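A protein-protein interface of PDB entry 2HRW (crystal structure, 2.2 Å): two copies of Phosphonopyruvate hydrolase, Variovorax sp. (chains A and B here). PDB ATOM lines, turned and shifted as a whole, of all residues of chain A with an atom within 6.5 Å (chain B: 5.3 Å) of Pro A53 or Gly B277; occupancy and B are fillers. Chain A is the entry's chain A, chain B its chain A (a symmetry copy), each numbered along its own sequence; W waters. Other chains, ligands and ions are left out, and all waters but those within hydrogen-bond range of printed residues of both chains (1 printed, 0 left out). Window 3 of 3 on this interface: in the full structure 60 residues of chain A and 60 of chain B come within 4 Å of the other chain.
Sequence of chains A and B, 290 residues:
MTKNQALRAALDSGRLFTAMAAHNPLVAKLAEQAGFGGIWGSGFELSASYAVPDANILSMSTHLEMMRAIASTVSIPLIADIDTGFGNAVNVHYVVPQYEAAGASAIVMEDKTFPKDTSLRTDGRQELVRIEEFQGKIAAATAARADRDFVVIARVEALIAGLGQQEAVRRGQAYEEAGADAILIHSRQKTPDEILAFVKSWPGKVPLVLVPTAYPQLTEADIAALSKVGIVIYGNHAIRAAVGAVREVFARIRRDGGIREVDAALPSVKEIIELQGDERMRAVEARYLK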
ATOM      1  N   SER A  47      -8.157  -1.027 -14.480  1.00  0.00           N
ATOM      2  CA  SER A  47      -9.078  -2.059 -14.059  1.00  0.00           C
ATOM      3  C   SER A  47     -10.099  -2.262 -15.165  1.00  0.00           C
ATOM      4  O   SER A  47     -10.686  -3.338 -15.292  1.00  0.00           O
ATOM      5  CB  SER A  47      -9.781  -1.640 -12.766  1.00  0.00           C
ATOM      6  OG  SER A  47     -10.458  -0.416 -12.969  1.00  0.00           O
ATOM      7  N   ALA A  48     -10.313  -1.222 -15.970  1.00  0.00           N
ATOM      8  CA  ALA A  48     -11.278  -1.318 -17.042  1.00  0.00           C
ATOM      9  C   ALA A  48     -10.674  -2.196 -18.145  1.00  0.00           C
ATOM     10  O   ALA A  48     -11.349  -3.070 -18.698  1.00  0.00           O
ATOM     11  CB  ALA A  48     -11.610   0.083 -17.561  1.00  0.00           C
ATOM     12  N   ALA A  51     -11.259  -5.625 -17.589  1.00  0.00           N
ATOM     13  CA  ALA A  51     -12.647  -6.047 -17.440  1.00  0.00           C
ATOM     14  C   ALA A  51     -13.001  -6.364 -15.984  1.00  0.00           C
ATOM     15  O   ALA A  51     -13.648  -7.366 -15.687  1.00  0.00           O
ATOM     16  CB  ALA A  51     -12.939  -7.262 -18.344  1.00  0.00           C
ATOM     17  N   VAL A  52     -12.540  -5.519 -15.068  1.00  0.00           N
ATOM     18  CA  VAL A  52     -12.901  -5.702 -13.667  1.00  0.00           C
ATOM     19  C   VAL A  52     -13.348  -4.362 -13.095  1.00  0.00           C
ATOM     20  O   VAL A  52     -12.837  -3.312 -13.477  1.00  0.00           O
ATOM     21  CB  VAL A  52     -11.748  -6.297 -12.801  1.00  0.00           C
ATOM     22  CG1 VAL A  52     -11.459  -7.723 -13.237  1.00  0.00           C
ATOM     23  CG2 VAL A  52     -10.506  -5.442 -12.916  1.00  0.00           C
ATOM     24  N   PRO A  53     -14.340  -4.393 -12.187  1.00  0.00           N
ATOM     25  CA  PRO A  53     -14.872  -3.188 -11.550  1.00  0.00           C
ATOM     26  C   PRO A  53     -13.736  -2.467 -10.855  1.00  0.00           C
ATOM     27  O   PRO A  53     -12.789  -3.089 -10.363  1.00  0.00           O
ATOM     28  CB  PRO A  53     -15.880  -3.735 -10.543  1.00  0.00           C
ATOM     29  CG  PRO A  53     -16.279  -5.060 -11.131  1.00  0.00           C
ATOM     30  CD  PRO A  53     -14.972  -5.598 -11.628  1.00  0.00           C
ATOM     31  N   ASP A  54     -13.836  -1.147 -10.828  1.00  0.00           N
ATOM     32  CA  ASP A  54     -12.824  -0.313 -10.203  1.00  0.00           C
ATOM     33  C   ASP A  54     -13.095  -0.194  -8.695  1.00  0.00           C
ATOM     34  O   ASP A  54     -13.332   0.895  -8.169  1.00  0.00           O
ATOM     35  CB  ASP A  54     -12.835   1.067 -10.862  1.00  0.00           C
ATOM     36  CG  ASP A  54     -11.848   2.012 -10.245  1.00  0.00           C
ATOM     37  OD1 ASP A  54     -11.975   3.225 -10.490  1.00  0.00           O
ATOM     38  OD2 ASP A  54     -10.943   1.554  -9.525  1.00  0.00           O
ATOM     39  N   ALA A  55     -13.048  -1.319  -7.995  1.00  0.00           N
ATOM     40  CA  ALA A  55     -13.296  -1.303  -6.572  1.00  0.00           C
ATOM     41  C   ALA A  55     -12.167  -2.007  -5.825  1.00  0.00           C
ATOM     42  O   ALA A  55     -12.416  -2.830  -4.941  1.00  0.00           O
ATOM     43  CB  ALA A  55     -14.620  -1.969  -6.280  1.00  0.00           C
ATOM     44  N   ASN A  56     -10.927  -1.660  -6.180  1.00  0.00           N
ATOM     45  CA  ASN A  56      -9.740  -2.256  -5.571  1.00  0.00           C
ATOM     46  C   ASN A  56      -9.667  -3.757  -5.847  1.00  0.00           C
ATOM     47  O   ASN A  56      -9.206  -4.530  -5.007  1.00  0.00           O
ATOM     48  CB  ASN A  56      -9.713  -2.017  -4.049  1.00  0.00           C
ATOM     49  CG  ASN A  56      -9.055  -0.690  -3.666  1.00  0.00           C
ATOM     50  OD1 ASN A  56      -7.870  -0.640  -3.293  1.00  0.00           O
ATOM     51  ND2 ASN A  56      -9.821   0.392  -3.760  1.00  0.00           N
ATOM     52  N   ILE A  57     -10.135  -4.174  -7.016  1.00  0.00           N
ATOM     53  CA  ILE A  57     -10.072  -5.588  -7.381  1.00  0.00           C
ATOM     54  C   ILE A  57      -8.656  -5.888  -7.894  1.00  0.00           C
ATOM     55  O   ILE A  57      -8.018  -6.826  -7.434  1.00  0.00           O
ATOM     56  CB  ILE A  57     -11.081  -5.937  -8.492  1.00  0.00           C
ATOM     57  CG1 ILE A  57     -12.501  -5.583  -8.036  1.00  0.00           C
ATOM     58  CG2 ILE A  57     -10.951  -7.406  -8.851  1.00  0.00           C
ATOM     59  CD1 ILE A  57     -12.965  -6.301  -6.782  1.00  0.00           C
ATOM     60  N   LEU A  58      -8.174  -5.090  -8.846  1.00  0.00           N
ATOM     61  CA  LEU A  58      -6.828  -5.281  -9.393  1.00  0.00           C
ATOM     62  C   LEU A  58      -5.787  -5.257  -8.293  1.00  0.00           C
ATOM     63  O   LEU A  58      -5.855  -4.421  -7.401  1.00  0.00           O
ATOM     64  CB  LEU A  58      -6.481  -4.172 -10.385  1.00  0.00           C
ATOM     65  CG  LEU A  58      -6.716  -4.389 -11.869  1.00  0.00           C
ATOM     66  CD1 LEU A  58      -6.171  -3.203 -12.625  1.00  0.00           C
ATOM     67  CD2 LEU A  58      -6.020  -5.650 -12.311  1.00  0.00           C
ATOM     68  N   LYS B  29     -12.461  -9.534 -24.579  1.00  0.00           N
ATOM     69  CA  LYS B  29     -13.888  -9.609 -24.267  1.00  0.00           C
ATOM     70  C   LYS B  29     -14.672  -9.067 -25.446  1.00  0.00           C
ATOM     71  O   LYS B  29     -15.635  -9.677 -25.900  1.00  0.00           O
ATOM     72  CB  LYS B  29     -14.192  -8.763 -23.045  1.00  0.00           C
ATOM     73  CG  LYS B  29     -15.651  -8.813 -22.572  1.00  0.00           C
ATOM     74  CD  LYS B  29     -15.755  -8.131 -21.218  1.00  0.00           C
ATOM     75  CE  LYS B  29     -17.057  -8.422 -20.517  1.00  0.00           C
ATOM     76  NZ  LYS B  29     -17.030  -7.876 -19.125  1.00  0.00           N
ATOM     77  N   ILE B 273     -17.985   0.901 -17.649  1.00  0.00           N
ATOM     78  CA  ILE B 273     -18.319   0.201 -16.396  1.00  0.00           C
ATOM     79  C   ILE B 273     -19.037  -1.139 -16.669  1.00  0.00           C
ATOM     80  O   ILE B 273     -18.786  -2.135 -15.983  1.00  0.00           O
ATOM     81  CB  ILE B 273     -19.212   1.079 -15.443  1.00  0.00           C
ATOM     82  CG1 ILE B 273     -18.344   2.025 -14.600  1.00  0.00           C
ATOM     83  CG2 ILE B 273     -19.979   0.213 -14.474  1.00  0.00           C
ATOM     84  CD1 ILE B 273     -17.669   3.091 -15.376  1.00  0.00           C
ATOM     85  N   GLU B 274     -19.917  -1.174 -17.671  1.00  0.00           N
ATOM     86  CA  GLU B 274     -20.632  -2.404 -18.005  1.00  0.00           C
ATOM     87  C   GLU B 274     -19.679  -3.476 -18.525  1.00  0.00           C
ATOM     88  O   GLU B 274     -19.861  -4.650 -18.250  1.00  0.00           O
ATOM     89  CB  GLU B 274     -21.702  -2.145 -19.069  1.00  0.00           C
ATOM     90  CG  GLU B 274     -22.537  -0.917 -18.816  1.00  0.00           C
ATOM     91  CD  GLU B 274     -23.646  -0.727 -19.857  1.00  0.00           C
ATOM     92  OE1 GLU B 274     -23.369  -0.894 -21.070  1.00  0.00           O
ATOM     93  OE2 GLU B 274     -24.794  -0.398 -19.451  1.00  0.00           O
ATOM     94  N   LEU B 275     -18.688  -3.065 -19.306  1.00  0.00           N
ATOM     95  CA  LEU B 275     -17.705  -3.997 -19.834  1.00  0.00           C
ATOM     96  C   LEU B 275     -16.777  -4.508 -18.726  1.00  0.00           C
ATOM     97  O   LEU B 275     -16.188  -5.572 -18.864  1.00  0.00           O
ATOM     98  CB  LEU B 275     -16.884  -3.325 -20.929  1.00  0.00           C
ATOM     99  CG  LEU B 275     -17.582  -3.254 -22.280  1.00  0.00           C
ATOM    100  CD1 LEU B 275     -17.113  -2.007 -22.967  1.00  0.00           C
ATOM    101  CD2 LEU B 275     -17.296  -4.528 -23.115  1.00  0.00           C
ATOM    102  N   GLN B 276     -16.647  -3.736 -17.642  1.00  0.00           N
ATOM    103  CA  GLN B 276     -15.829  -4.131 -16.493  1.00  0.00           C
ATOM    104  C   GLN B 276     -16.493  -5.239 -15.663  1.00  0.00           C
ATOM    105  O   GLN B 276     -15.868  -5.846 -14.798  1.00  0.00           O
ATOM    106  CB  GLN B 276     -15.562  -2.924 -15.596  1.00  0.00           C
ATOM    107  CG  GLN B 276     -14.460  -2.025 -16.093  1.00  0.00           C
ATOM    108  CD  GLN B 276     -14.241  -0.842 -15.184  1.00  0.00           C
ATOM    109  OE1 GLN B 276     -15.107   0.017 -15.036  1.00  0.00           O
ATOM    110  NE2 GLN B 276     -13.079  -0.792 -14.564  1.00  0.00           N
ATOM    111  N   GLY B 277     -17.769  -5.497 -15.927  1.00  0.00           N
ATOM    112  CA  GLY B 277     -18.462  -6.544 -15.199  1.00  0.00           C
ATOM    113  C   GLY B 277     -19.151  -5.977 -13.979  1.00  0.00           C
ATOM    114  O   GLY B 277     -19.177  -6.600 -12.908  1.00  0.00           O
ATOM    115  N   ASP B 278     -19.723  -4.789 -14.142  1.00  0.00           N
ATOM    116  CA  ASP B 278     -20.401  -4.140 -13.037  1.00  0.00           C
ATOM    117  C   ASP B 278     -21.596  -4.915 -12.506  1.00  0.00           C
ATOM    118  O   ASP B 278     -21.876  -4.883 -11.306  1.00  0.00           O
ATOM    119  CB  ASP B 278     -20.878  -2.765 -13.441  1.00  0.00           C
ATOM    120  CG  ASP B 278     -21.478  -2.014 -12.280  1.00  0.00           C
ATOM    121  OD1 ASP B 278     -20.694  -1.593 -11.388  1.00  0.00           O
ATOM    122  OD2 ASP B 278     -22.730  -1.871 -12.265  1.00  0.00           O
ATOM    123  N   GLU B 279     -22.305  -5.584 -13.413  1.00  0.00           N
ATOM    124  CA  GLU B 279     -23.477  -6.373 -13.085  1.00  0.00           C
ATOM    125  C   GLU B 279     -23.101  -7.459 -12.096  1.00  0.00           C
ATOM    126  O   GLU B 279     -23.753  -7.629 -11.070  1.00  0.00           O
ATOM    127  CB  GLU B 279     -24.054  -6.994 -14.351  1.00  0.00           C
ATOM    128  N   ARG B 280     -22.049  -8.203 -12.404  1.00  0.00           N
ATOM    129  CA  ARG B 280     -21.622  -9.244 -11.501  1.00  0.00           C
ATOM    130  C   ARG B 280     -21.301  -8.610 -10.152  1.00  0.00           C
ATOM    131  O   ARG B 280     -21.681  -9.142  -9.105  1.00  0.00           O
ATOM    132  CB  ARG B 280     -20.383  -9.965 -12.035  1.00  0.00           C
ATOM    133  CG  ARG B 280     -19.768 -10.937 -11.013  1.00  0.00           C
ATOM    134  CD  ARG B 280     -18.441 -11.498 -11.483  1.00  0.00           C
ATOM    135  NE  ARG B 280     -17.624 -11.977 -10.375  1.00  0.00           N
ATOM    136  CZ  ARG B 280     -16.351 -12.361 -10.486  1.00  0.00           C
ATOM    137  NH1 ARG B 280     -15.734 -12.332 -11.665  1.00  0.00           N
ATOM    138  NH2 ARG B 280     -15.679 -12.743  -9.405  1.00  0.00           N
ATOM    139  N   MET B 281     -20.611  -7.467 -10.170  1.00  0.00           N
ATOM    140  CA  MET B 281     -20.249  -6.815  -8.917  1.00  0.00           C
ATOM    141  C   MET B 281     -21.441  -6.331  -8.097  1.00  0.00           C
ATOM    142  O   MET B 281     -21.388  -6.361  -6.865  1.00  0.00           O
ATOM    143  CB  MET B 281     -19.298  -5.644  -9.145  1.00  0.00           C
ATOM    144  CG  MET B 281     -18.742  -5.151  -7.830  1.00  0.00           C
ATOM    145  SD  MET B 281     -17.329  -4.082  -7.937  1.00  0.00           S
ATOM    146  CE  MET B 281     -18.138  -2.496  -7.612  1.00  0.00           C
HETATM  147  O   HOH W   1     -15.990  -0.009 -12.111  1.00  0.00           O
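No position is printed for both chains.
Printed residues of chain B within 4 Å of Ala A51: Leu B275 (3.7 Å) and Gln B276 (2.8 Å). Pro A53 touches just these residues of chain B: Gln B276, Gly B277 and Met B281. Of the printed residues of chain B, Asp A54 touches Gln B276 (3.8 Å). Asn A56 touches none of the printed residues of chain B. Leu A58 touches none of the printed residues of chain B. Of the printed residues of chain A, Gln B276 touches Ser A47, Ala A48, Ala A51, Val A52, Pro A53 and Asp A54. Gly B277 touches just one residue of chain A: Pro A53. The nearest residue of chain B that does not touch Pro A53 is Asp B278 (4.6 Å). The nearest residue of chain A that does not touch Gly B277 is Ala A51 (4.5 Å). The nearest printed residue of chain B that does not touch Ser A47 is Leu B275 (6.9 Å).
The side-chain hydroxyl of Ser A47 lies within hydrogen-bond range of the side-chain amide nitrogen of Gln B276, 3.1 Å away. The backbone NH of Ala A48 sits close to the side-chain amide nitrogen of Gln B276 (3.1 Å). The backbone carbonyl oxygen of Val A52 lies within hydrogen-bond range of the side-chain amide nitrogen of Gln B276 (2.8 Å). The backbone carbonyl oxygen (O) of Ala A51 sits close to the backbone carbonyl oxygen (O) of Gln B276 (2.8 Å). N of Pro A53 lies close to O of Gln B276, at 3.4 Å.
Water W1 bridges N of Asp A54 (2.8 Å) and OE1 of Gln B276 (3.1 Å).
The backbone carbonyl oxygen of Ser A47 is in hydrogen-bond range of the backbone NH of Val A52 (2.9 Å). The side-chain amino group (NZ) of Lys B29 lies within hydrogen-bond range of the backbone carbonyl oxygen (O) of Leu B275.
CB of Ala A51 touches O of Leu B275, at 3.7 Å. Pro A53 touches Gly B277. CB of Pro A53 touches SD of Met B281 (3.0 Å). Asp A54 touches Gln B276 (N to NE2, 3.8 Å). Met B281 touches Ala A55 (CE to CB, 3.8 Å).
Hydrophobic or aromatic side chains of chain B within 4 Å of the printed part of chain A: Met B281. Hydrophobic or aromatic side chains of chain A that line the printed part of chain B: Ala A48, Ala A51, Pro A53 and Ala A55. Among the printed residues, 10 pairs touch across the chains. Among the printed residues, no Asp or Glu carboxylate lies within 4 Å of a Lys or Arg side-chain nitrogen of the other chain.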
